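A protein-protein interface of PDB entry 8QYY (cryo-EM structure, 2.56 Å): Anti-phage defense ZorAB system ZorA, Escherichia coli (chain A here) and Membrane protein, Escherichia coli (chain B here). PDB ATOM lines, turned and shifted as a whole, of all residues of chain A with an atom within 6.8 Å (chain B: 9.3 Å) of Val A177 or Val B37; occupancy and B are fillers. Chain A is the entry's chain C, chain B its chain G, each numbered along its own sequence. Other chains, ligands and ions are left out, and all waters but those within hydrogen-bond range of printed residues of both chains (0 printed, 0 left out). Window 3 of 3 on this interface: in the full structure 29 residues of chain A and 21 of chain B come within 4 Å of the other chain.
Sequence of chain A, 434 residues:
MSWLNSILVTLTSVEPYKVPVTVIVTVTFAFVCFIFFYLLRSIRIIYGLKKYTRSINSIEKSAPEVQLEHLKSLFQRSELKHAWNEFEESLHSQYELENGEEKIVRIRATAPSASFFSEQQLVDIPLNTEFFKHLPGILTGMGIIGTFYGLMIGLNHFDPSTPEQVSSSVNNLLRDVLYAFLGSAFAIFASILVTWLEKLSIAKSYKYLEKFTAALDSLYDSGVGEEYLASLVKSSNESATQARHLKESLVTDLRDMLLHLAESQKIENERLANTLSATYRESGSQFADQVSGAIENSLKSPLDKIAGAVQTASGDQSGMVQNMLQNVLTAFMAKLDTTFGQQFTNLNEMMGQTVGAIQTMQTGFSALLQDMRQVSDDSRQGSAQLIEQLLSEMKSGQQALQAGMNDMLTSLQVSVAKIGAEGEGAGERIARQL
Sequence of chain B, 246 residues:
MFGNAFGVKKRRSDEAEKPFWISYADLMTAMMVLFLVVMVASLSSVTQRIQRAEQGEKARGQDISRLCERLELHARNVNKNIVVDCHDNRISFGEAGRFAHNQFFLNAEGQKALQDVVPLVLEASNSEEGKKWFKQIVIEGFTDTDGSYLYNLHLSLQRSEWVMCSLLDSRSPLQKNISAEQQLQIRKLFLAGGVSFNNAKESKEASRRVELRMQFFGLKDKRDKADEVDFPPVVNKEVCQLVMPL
The side-chain hydroxyl of Ser B45 lies within hydrogen-bond range of the backbone carbonyl oxygen of Ala B41.
Leu A151 touches Val B33. Ala B41 touches Val A170 (CB to CG1, 3.6 Å). Leu A174 touches Val B37 (CD2 to CG1, 3.6 Å). Val A177 touches Val B33 (CG2 to CG1, 3.7 Å). Val A177 touches Val B37 (CG2 to CG2, 3.5 Å). Phe A181 touches Ala B30 (CE1 to O, 3.4 Å). Phe A181 touches Leu B34.
Gly A150 touches none of the printed residues of chain B. Printed residues of chain B within 4 Å of Leu A151: Val B33. Leu A155 touches none of the printed residues of chain B. Of the printed residues of chain B, Leu A174 touches Val B37 (3.6 Å). Of chain B, only Val B33 and Val B37 come within 4 Å of Val A177. Printed residues of chain B within 4 Å of Phe A181: Ala B30 and Leu B34. Of the printed residues of chain A, Val B33 touches Leu A151 (3.4 Å) and Val A177 (3.7 Å). Printed residues of chain A within 4 Å of Ala B41: Val A170. The nearest residue of chain B that does not touch Val A177 is Leu B34 (4.3 Å).
Of the 16 printed residues of chain A, 5 touch a printed residue of chain B. Of the 17 printed residues of chain B, 5 touch a printed residue of chain A. Hydrophobic or aromatic side chains of chain B within 4 Å of the printed part of chain A: Ala B30, Val B33, Leu B34, Val B37 and Ala B41. Among the printed residues, 7 pairs touch across the chains.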
ATOM      1  N   THR A 147      20.873  14.284 -14.219  1.00  0.00           N
ATOM      2  CA  THR A 147      21.804  15.370 -14.522  1.00  0.00           C
ATOM      3  C   THR A 147      21.098  16.505 -15.256  1.00  0.00           C
ATOM      4  O   THR A 147      21.167  17.674 -14.847  1.00  0.00           O
ATOM      5  CB  THR A 147      22.972  14.839 -15.353  1.00  0.00           C
ATOM      6  OG1 THR A 147      23.852  14.082 -14.515  1.00  0.00           O
ATOM      7  CG2 THR A 147      23.749  15.982 -15.988  1.00  0.00           C
ATOM      8  N   GLY A 150      18.394  18.303 -12.945  1.00  0.00           N
ATOM      9  CA  GLY A 150      18.999  19.158 -11.943  1.00  0.00           C
ATOM     10  C   GLY A 150      19.571  20.427 -12.541  1.00  0.00           C
ATOM     11  O   GLY A 150      19.424  21.517 -11.977  1.00  0.00           O
ATOM     12  N   LEU A 151      20.218  20.310 -13.701  1.00  0.00           N
ATOM     13  CA  LEU A 151      20.740  21.516 -14.332  1.00  0.00           C
ATOM     14  C   LEU A 151      19.626  22.414 -14.848  1.00  0.00           C
ATOM     15  O   LEU A 151      19.770  23.637 -14.840  1.00  0.00           O
ATOM     16  CB  LEU A 151      21.721  21.169 -15.445  1.00  0.00           C
ATOM     17  CG  LEU A 151      23.141  20.976 -14.919  1.00  0.00           C
ATOM     18  CD1 LEU A 151      23.612  22.302 -14.333  1.00  0.00           C
ATOM     19  CD2 LEU A 151      23.304  19.850 -13.906  1.00  0.00           C
ATOM     20  N   LEU A 155      19.428  26.281 -13.831  1.00  0.00           N
ATOM     21  CA  LEU A 155      19.487  27.329 -14.843  1.00  0.00           C
ATOM     22  C   LEU A 155      18.234  28.195 -14.827  1.00  0.00           C
ATOM     23  O   LEU A 155      18.319  29.417 -14.986  1.00  0.00           O
ATOM     24  CB  LEU A 155      19.684  26.709 -16.224  1.00  0.00           C
ATOM     25  CG  LEU A 155      21.004  25.985 -16.495  1.00  0.00           C
ATOM     26  CD1 LEU A 155      20.819  24.933 -17.569  1.00  0.00           C
ATOM     27  CD2 LEU A 155      22.082  26.960 -16.894  1.00  0.00           C
ATOM     28  N   VAL A 170      24.872  31.316  -8.503  1.00  0.00           N
ATOM     29  CA  VAL A 170      26.061  30.562  -8.885  1.00  0.00           C
ATOM     30  C   VAL A 170      26.323  29.434  -7.892  1.00  0.00           C
ATOM     31  O   VAL A 170      26.696  28.319  -8.279  1.00  0.00           O
ATOM     32  CB  VAL A 170      27.266  31.510  -9.010  1.00  0.00           C
ATOM     33  CG1 VAL A 170      28.558  30.732  -9.015  1.00  0.00           C
ATOM     34  CG2 VAL A 170      27.143  32.350 -10.264  1.00  0.00           C
ATOM     35  N   ASN A 172      24.031  27.897  -6.175  1.00  0.00           N
ATOM     36  CA  ASN A 172      23.017  26.894  -6.479  1.00  0.00           C
ATOM     37  C   ASN A 172      23.399  26.084  -7.709  1.00  0.00           C
ATOM     38  O   ASN A 172      23.184  24.870  -7.749  1.00  0.00           O
ATOM     39  CB  ASN A 172      21.656  27.561  -6.676  1.00  0.00           C
ATOM     40  CG  ASN A 172      21.154  28.240  -5.421  1.00  0.00           C
ATOM     41  OD1 ASN A 172      21.582  27.922  -4.314  1.00  0.00           O
ATOM     42  ND2 ASN A 172      20.231  29.179  -5.587  1.00  0.00           N
ATOM     43  N   LEU A 173      23.962  26.739  -8.725  1.00  0.00           N
ATOM     44  CA  LEU A 173      24.409  26.018  -9.916  1.00  0.00           C
ATOM     45  C   LEU A 173      25.515  25.025  -9.582  1.00  0.00           C
ATOM     46  O   LEU A 173      25.513  23.892 -10.075  1.00  0.00           O
ATOM     47  CB  LEU A 173      24.884  27.005 -10.980  1.00  0.00           C
ATOM     48  CG  LEU A 173      23.904  27.303 -12.112  1.00  0.00           C
ATOM     49  CD1 LEU A 173      24.501  28.309 -13.071  1.00  0.00           C
ATOM     50  CD2 LEU A 173      23.533  26.027 -12.839  1.00  0.00           C
ATOM     51  N   LEU A 174      26.475  25.438  -8.753  1.00  0.00           N
ATOM     52  CA  LEU A 174      27.548  24.530  -8.364  1.00  0.00           C
ATOM     53  C   LEU A 174      27.012  23.346  -7.566  1.00  0.00           C
ATOM     54  O   LEU A 174      27.421  22.199  -7.790  1.00  0.00           O
ATOM     55  CB  LEU A 174      28.611  25.288  -7.571  1.00  0.00           C
ATOM     56  CG  LEU A 174      29.438  26.292  -8.374  1.00  0.00           C
ATOM     57  CD1 LEU A 174      30.238  27.191  -7.452  1.00  0.00           C
ATOM     58  CD2 LEU A 174      30.358  25.572  -9.336  1.00  0.00           C
ATOM     59  N   ARG A 175      26.083  23.600  -6.637  1.00  0.00           N
ATOM     60  CA  ARG A 175      25.480  22.502  -5.887  1.00  0.00           C
ATOM     61  C   ARG A 175      24.707  21.568  -6.806  1.00  0.00           C
ATOM     62  O   ARG A 175      24.716  20.351  -6.610  1.00  0.00           O
ATOM     63  CB  ARG A 175      24.564  23.036  -4.788  1.00  0.00           C
ATOM     64  CG  ARG A 175      25.258  23.872  -3.733  1.00  0.00           C
ATOM     65  CD  ARG A 175      26.235  23.063  -2.892  1.00  0.00           C
ATOM     66  NE  ARG A 175      25.569  22.033  -2.103  1.00  0.00           N
ATOM     67  CZ  ARG A 175      26.190  21.011  -1.532  1.00  0.00           C
ATOM     68  NH1 ARG A 175      27.501  20.862  -1.619  1.00  0.00           N
ATOM     69  NH2 ARG A 175      25.479  20.120  -0.849  1.00  0.00           N
ATOM     70  N   ASP A 176      24.030  22.119  -7.812  1.00  0.00           N
ATOM     71  CA  ASP A 176      23.279  21.287  -8.745  1.00  0.00           C
ATOM     72  C   ASP A 176      24.200  20.423  -9.594  1.00  0.00           C
ATOM     73  O   ASP A 176      23.881  19.263  -9.876  1.00  0.00           O
ATOM     74  CB  ASP A 176      22.392  22.162  -9.623  1.00  0.00           C
ATOM     75  CG  ASP A 176      21.257  22.785  -8.849  1.00  0.00           C
ATOM     76  OD1 ASP A 176      20.806  22.167  -7.864  1.00  0.00           O
ATOM     77  OD2 ASP A 176      20.824  23.896  -9.206  1.00  0.00           O
ATOM     78  N   VAL A 177      25.344  20.960 -10.012  1.00  0.00           N
ATOM     79  CA  VAL A 177      26.288  20.145 -10.773  1.00  0.00           C
ATOM     80  C   VAL A 177      26.886  19.055  -9.891  1.00  0.00           C
ATOM     81  O   VAL A 177      27.080  17.917 -10.334  1.00  0.00           O
ATOM     82  CB  VAL A 177      27.376  21.022 -11.417  1.00  0.00           C
ATOM     83  CG1 VAL A 177      28.286  20.177 -12.276  1.00  0.00           C
ATOM     84  CG2 VAL A 177      26.743  22.084 -12.264  1.00  0.00           C
ATOM     85  N   LEU A 178      27.182  19.377  -8.629  1.00  0.00           N
ATOM     86  CA  LEU A 178      27.656  18.355  -7.699  1.00  0.00           C
ATOM     87  C   LEU A 178      26.610  17.262  -7.504  1.00  0.00           C
ATOM     88  O   LEU A 178      26.935  16.068  -7.473  1.00  0.00           O
ATOM     89  CB  LEU A 178      28.015  18.999  -6.363  1.00  0.00           C
ATOM     90  CG  LEU A 178      28.745  18.123  -5.350  1.00  0.00           C
ATOM     91  CD1 LEU A 178      30.163  17.862  -5.808  1.00  0.00           C
ATOM     92  CD2 LEU A 178      28.738  18.789  -3.994  1.00  0.00           C
ATOM     93  N   TYR A 179      25.345  17.660  -7.373  1.00  0.00           N
ATOM     94  CA  TYR A 179      24.250  16.707  -7.252  1.00  0.00           C
ATOM     95  C   TYR A 179      24.143  15.819  -8.483  1.00  0.00           C
ATOM     96  O   TYR A 179      23.906  14.611  -8.373  1.00  0.00           O
ATOM     97  CB  TYR A 179      22.944  17.469  -7.039  1.00  0.00           C
ATOM     98  CG  TYR A 179      22.749  18.032  -5.653  1.00  0.00           C
ATOM     99  CD1 TYR A 179      23.540  17.618  -4.594  1.00  0.00           C
ATOM    100  CD2 TYR A 179      21.767  18.978  -5.405  1.00  0.00           C
ATOM    101  CE1 TYR A 179      23.359  18.134  -3.330  1.00  0.00           C
ATOM    102  CE2 TYR A 179      21.579  19.496  -4.146  1.00  0.00           C
ATOM    103  CZ  TYR A 179      22.377  19.069  -3.110  1.00  0.00           C
ATOM    104  OH  TYR A 179      22.195  19.583  -1.849  1.00  0.00           O
ATOM    105  N   ALA A 180      24.281  16.411  -9.671  1.00  0.00           N
ATOM    106  CA  ALA A 180      24.212  15.635 -10.902  1.00  0.00           C
ATOM    107  C   ALA A 180      25.356  14.638 -10.989  1.00  0.00           C
ATOM    108  O   ALA A 180      25.163  13.494 -11.416  1.00  0.00           O
ATOM    109  CB  ALA A 180      24.216  16.569 -12.110  1.00  0.00           C
ATOM    110  N   PHE A 181      26.558  15.055 -10.587  1.00  0.00           N
ATOM    111  CA  PHE A 181      27.687  14.132 -10.554  1.00  0.00           C
ATOM    112  C   PHE A 181      27.418  12.978  -9.598  1.00  0.00           C
ATOM    113  O   PHE A 181      27.713  11.821  -9.913  1.00  0.00           O
ATOM    114  CB  PHE A 181      28.964  14.856 -10.134  1.00  0.00           C
ATOM    115  CG  PHE A 181      29.508  15.799 -11.159  1.00  0.00           C
ATOM    116  CD1 PHE A 181      28.888  15.968 -12.381  1.00  0.00           C
ATOM    117  CD2 PHE A 181      30.658  16.517 -10.900  1.00  0.00           C
ATOM    118  CE1 PHE A 181      29.399  16.843 -13.310  1.00  0.00           C
ATOM    119  CE2 PHE A 181      31.174  17.387 -11.828  1.00  0.00           C
ATOM    120  CZ  PHE A 181      30.545  17.547 -13.034  1.00  0.00           C
ATOM    121  N   LEU A 182      26.869  13.279  -8.421  1.00  0.00           N
ATOM    122  CA  LEU A 182      26.576  12.233  -7.445  1.00  0.00           C
ATOM    123  C   LEU A 182      25.547  11.248  -7.983  1.00  0.00           C
ATOM    124  O   LEU A 182      25.706  10.028  -7.853  1.00  0.00           O
ATOM    125  CB  LEU A 182      26.083  12.866  -6.146  1.00  0.00           C
ATOM    126  CG  LEU A 182      25.488  11.923  -5.102  1.00  0.00           C
ATOM    127  CD1 LEU A 182      26.580  11.131  -4.405  1.00  0.00           C
ATOM    128  CD2 LEU A 182      24.660  12.706  -4.102  1.00  0.00           C
ATOM    129  N   THR B  29      28.515  14.636 -20.945  1.00  0.00           N
ATOM    130  CA  THR B  29      27.536  15.644 -20.559  1.00  0.00           C
ATOM    131  C   THR B  29      27.901  16.280 -19.225  1.00  0.00           C
ATOM    132  O   THR B  29      27.780  17.497 -19.055  1.00  0.00           O
ATOM    133  CB  THR B  29      26.145  15.023 -20.488  1.00  0.00           C
ATOM    134  OG1 THR B  29      25.855  14.365 -21.725  1.00  0.00           O
ATOM    135  CG2 THR B  29      25.107  16.093 -20.235  1.00  0.00           C
ATOM    136  N   ALA B  30      28.347  15.467 -18.266  1.00  0.00           N
ATOM    137  CA  ALA B  30      28.743  15.997 -16.969  1.00  0.00           C
ATOM    138  C   ALA B  30      29.929  16.943 -17.096  1.00  0.00           C
ATOM    139  O   ALA B  30      29.972  17.986 -16.440  1.00  0.00           O
ATOM    140  CB  ALA B  30      29.071  14.847 -16.023  1.00  0.00           C
ATOM    141  N   MET B  31      30.901  16.591 -17.935  1.00  0.00           N
ATOM    142  CA  MET B  31      32.044  17.469 -18.167  1.00  0.00           C
ATOM    143  C   MET B  31      31.638  18.762 -18.863  1.00  0.00           C
ATOM    144  O   MET B  31      32.141  19.839 -18.523  1.00  0.00           O
ATOM    145  CB  MET B  31      33.103  16.734 -18.982  1.00  0.00           C
ATOM    146  CG  MET B  31      33.773  15.615 -18.250  1.00  0.00           C
ATOM    147  SD  MET B  31      34.570  16.337 -16.819  1.00  0.00           S
ATOM    148  CE  MET B  31      35.812  17.316 -17.642  1.00  0.00           C
ATOM    149  N   MET B  32      30.746  18.673 -19.846  1.00  0.00           N
ATOM    150  CA  MET B  32      30.251  19.869 -20.516  1.00  0.00           C
ATOM    151  C   MET B  32      29.548  20.794 -19.531  1.00  0.00           C
ATOM    152  O   MET B  32      29.770  22.012 -19.537  1.00  0.00           O
ATOM    153  CB  MET B  32      29.323  19.439 -21.655  1.00  0.00           C
ATOM    154  CG  MET B  32      28.738  20.530 -22.525  1.00  0.00           C
ATOM    155  SD  MET B  32      27.288  21.301 -21.787  1.00  0.00           S
ATOM    156  CE  MET B  32      26.104  19.975 -21.985  1.00  0.00           C
ATOM    157  N   VAL B  33      28.719  20.226 -18.656  1.00  0.00           N
ATOM    158  CA  VAL B  33      28.055  21.009 -17.620  1.00  0.00           C
ATOM    159  C   VAL B  33      29.063  21.623 -16.661  1.00  0.00           C
ATOM    160  O   VAL B  33      28.929  22.785 -16.259  1.00  0.00           O
ATOM    161  CB  VAL B  33      27.031  20.141 -16.873  1.00  0.00           C
ATOM    162  CG1 VAL B  33      26.465  20.921 -15.741  1.00  0.00           C
ATOM    163  CG2 VAL B  33      25.918  19.733 -17.812  1.00  0.00           C
ATOM    164  N   LEU B  34      30.063  20.844 -16.250  1.00  0.00           N
ATOM    165  CA  LEU B  34      31.072  21.362 -15.340  1.00  0.00           C
ATOM    166  C   LEU B  34      31.785  22.558 -15.946  1.00  0.00           C
ATOM    167  O   LEU B  34      31.982  23.576 -15.275  1.00  0.00           O
ATOM    168  CB  LEU B  34      32.079  20.266 -14.990  1.00  0.00           C
ATOM    169  CG  LEU B  34      33.334  20.698 -14.232  1.00  0.00           C
ATOM    170  CD1 LEU B  34      33.019  20.929 -12.767  1.00  0.00           C
ATOM    171  CD2 LEU B  34      34.438  19.673 -14.387  1.00  0.00           C
ATOM    172  N   PHE B  35      32.156  22.466 -17.221  1.00  0.00           N
ATOM    173  CA  PHE B  35      32.886  23.563 -17.846  1.00  0.00           C
ATOM    174  C   PHE B  35      31.997  24.785 -18.037  1.00  0.00           C
ATOM    175  O   PHE B  35      32.439  25.916 -17.812  1.00  0.00           O
ATOM    176  CB  PHE B  35      33.488  23.097 -19.166  1.00  0.00           C
ATOM    177  CG  PHE B  35      34.690  22.224 -18.990  1.00  0.00           C
ATOM    178  CD1 PHE B  35      35.488  22.357 -17.870  1.00  0.00           C
ATOM    179  CD2 PHE B  35      35.010  21.257 -19.921  1.00  0.00           C
ATOM    180  CE1 PHE B  35      36.592  21.553 -17.690  1.00  0.00           C
ATOM    181  CE2 PHE B  35      36.115  20.453 -19.744  1.00  0.00           C
ATOM    182  CZ  PHE B  35      36.904  20.599 -18.628  1.00  0.00           C
ATOM    183  N   LEU B  36      30.734  24.577 -18.417  1.00  0.00           N
ATOM    184  CA  LEU B  36      29.789  25.689 -18.477  1.00  0.00           C
ATOM    185  C   LEU B  36      29.669  26.406 -17.142  1.00  0.00           C
ATOM    186  O   LEU B  36      29.787  27.635 -17.068  1.00  0.00           O
ATOM    187  CB  LEU B  36      28.419  25.188 -18.916  1.00  0.00           C
ATOM    188  CG  LEU B  36      27.375  26.302 -18.969  1.00  0.00           C
ATOM    189  CD1 LEU B  36      27.722  27.378 -19.974  1.00  0.00           C
ATOM    190  CD2 LEU B  36      26.023  25.709 -19.250  1.00  0.00           C
ATOM    191  N   VAL B  37      29.407  25.653 -16.075  1.00  0.00           N
ATOM    192  CA  VAL B  37      29.143  26.279 -14.788  1.00  0.00           C
ATOM    193  C   VAL B  37      30.406  26.906 -14.222  1.00  0.00           C
ATOM    194  O   VAL B  37      30.344  27.944 -13.553  1.00  0.00           O
ATOM    195  CB  VAL B  37      28.508  25.257 -13.829  1.00  0.00           C
ATOM    196  CG1 VAL B  37      28.433  25.810 -12.422  1.00  0.00           C
ATOM    197  CG2 VAL B  37      27.126  24.900 -14.325  1.00  0.00           C
ATOM    198  N   VAL B  38      31.570  26.316 -14.487  1.00  0.00           N
ATOM    199  CA  VAL B  38      32.811  26.913 -14.019  1.00  0.00           C
ATOM    200  C   VAL B  38      33.090  28.209 -14.769  1.00  0.00           C
ATOM    201  O   VAL B  38      33.552  29.191 -14.179  1.00  0.00           O
ATOM    202  CB  VAL B  38      33.968  25.908 -14.151  1.00  0.00           C
ATOM    203  CG1 VAL B  38      35.310  26.609 -14.054  1.00  0.00           C
ATOM    204  CG2 VAL B  38      33.841  24.845 -13.091  1.00  0.00           C
ATOM    205  N   MET B  39      32.792  28.246 -16.071  1.00  0.00           N
ATOM    206  CA  MET B  39      32.894  29.499 -16.808  1.00  0.00           C
ATOM    207  C   MET B  39      31.962  30.553 -16.235  1.00  0.00           C
ATOM    208  O   MET B  39      32.352  31.713 -16.067  1.00  0.00           O
ATOM    209  CB  MET B  39      32.576  29.271 -18.284  1.00  0.00           C
ATOM    210  CG  MET B  39      32.708  30.517 -19.134  1.00  0.00           C
ATOM    211  SD  MET B  39      32.353  30.204 -20.864  1.00  0.00           S
ATOM    212  CE  MET B  39      30.589  29.971 -20.785  1.00  0.00           C
ATOM    213  N   VAL B  40      30.724  30.167 -15.932  1.00  0.00           N
ATOM    214  CA  VAL B  40      29.751  31.120 -15.401  1.00  0.00           C
ATOM    215  C   VAL B  40      30.225  31.672 -14.063  1.00  0.00           C
ATOM    216  O   VAL B  40      30.202  32.885 -13.830  1.00  0.00           O
ATOM    217  CB  VAL B  40      28.369  30.453 -15.280  1.00  0.00           C
ATOM    218  CG1 VAL B  40      27.457  31.271 -14.383  1.00  0.00           C
ATOM    219  CG2 VAL B  40      27.758  30.272 -16.650  1.00  0.00           C
ATOM    220  N   ALA B  41      30.674  30.786 -13.173  1.00  0.00           N
ATOM    221  CA  ALA B  41      31.147  31.217 -11.862  1.00  0.00           C
ATOM    222  C   ALA B  41      32.380  32.103 -11.977  1.00  0.00           C
ATOM    223  O   ALA B  41      32.481  33.129 -11.299  1.00  0.00           O
ATOM    224  CB  ALA B  41      31.443  30.000 -10.988  1.00  0.00           C
ATOM    225  N   SER B  42      33.328  31.727 -12.836  1.00  0.00           N
ATOM    226  CA  SER B  42      34.548  32.509 -12.980  1.00  0.00           C
ATOM    227  C   SER B  42      34.259  33.890 -13.549  1.00  0.00           C
ATOM    228  O   SER B  42      34.813  34.888 -13.073  1.00  0.00           O
ATOM    229  CB  SER B  42      35.539  31.757 -13.863  1.00  0.00           C
ATOM    230  OG  SER B  42      35.697  30.424 -13.421  1.00  0.00           O
ATOM    231  N   LEU B  43      33.401  33.968 -14.567  1.00  0.00           N
ATOM    232  CA  LEU B  43      33.067  35.263 -15.149  1.00  0.00           C
ATOM    233  C   LEU B  43      32.288  36.124 -14.167  1.00  0.00           C
ATOM    234  O   LEU B  43      32.507  37.336 -14.092  1.00  0.00           O
ATOM    235  CB  LEU B  43      32.282  35.071 -16.443  1.00  0.00           C
ATOM    236  CG  LEU B  43      33.094  34.546 -17.624  1.00  0.00           C
ATOM    237  CD1 LEU B  43      32.224  34.416 -18.857  1.00  0.00           C
ATOM    238  CD2 LEU B  43      34.274  35.453 -17.895  1.00  0.00           C
ATOM    239  N   SER B  44      31.373  35.521 -13.406  1.00  0.00           N
ATOM    240  CA  SER B  44      30.644  36.276 -12.397  1.00  0.00           C
ATOM    241  C   SER B  44      31.537  36.702 -11.242  1.00  0.00           C
ATOM    242  O   SER B  44      31.203  37.663 -10.541  1.00  0.00           O
ATOM    243  CB  SER B  44      29.470  35.450 -11.875  1.00  0.00           C
ATOM    244  OG  SER B  44      28.647  35.019 -12.941  1.00  0.00           O
ATOM    245  N   SER B  45      32.653  36.009 -11.023  1.00  0.00           N
ATOM    246  CA  SER B  45      33.555  36.382  -9.942  1.00  0.00           C
ATOM    247  C   SER B  45      34.518  37.486 -10.364  1.00  0.00           C
ATOM    248  O   SER B  45      34.766  38.421  -9.599  1.00  0.00           O
ATOM    249  CB  SER B  45      34.322  35.155  -9.456  1.00  0.00           C
ATOM    250  OG  SER B  45      33.430  34.113  -9.105  1.00  0.00           O
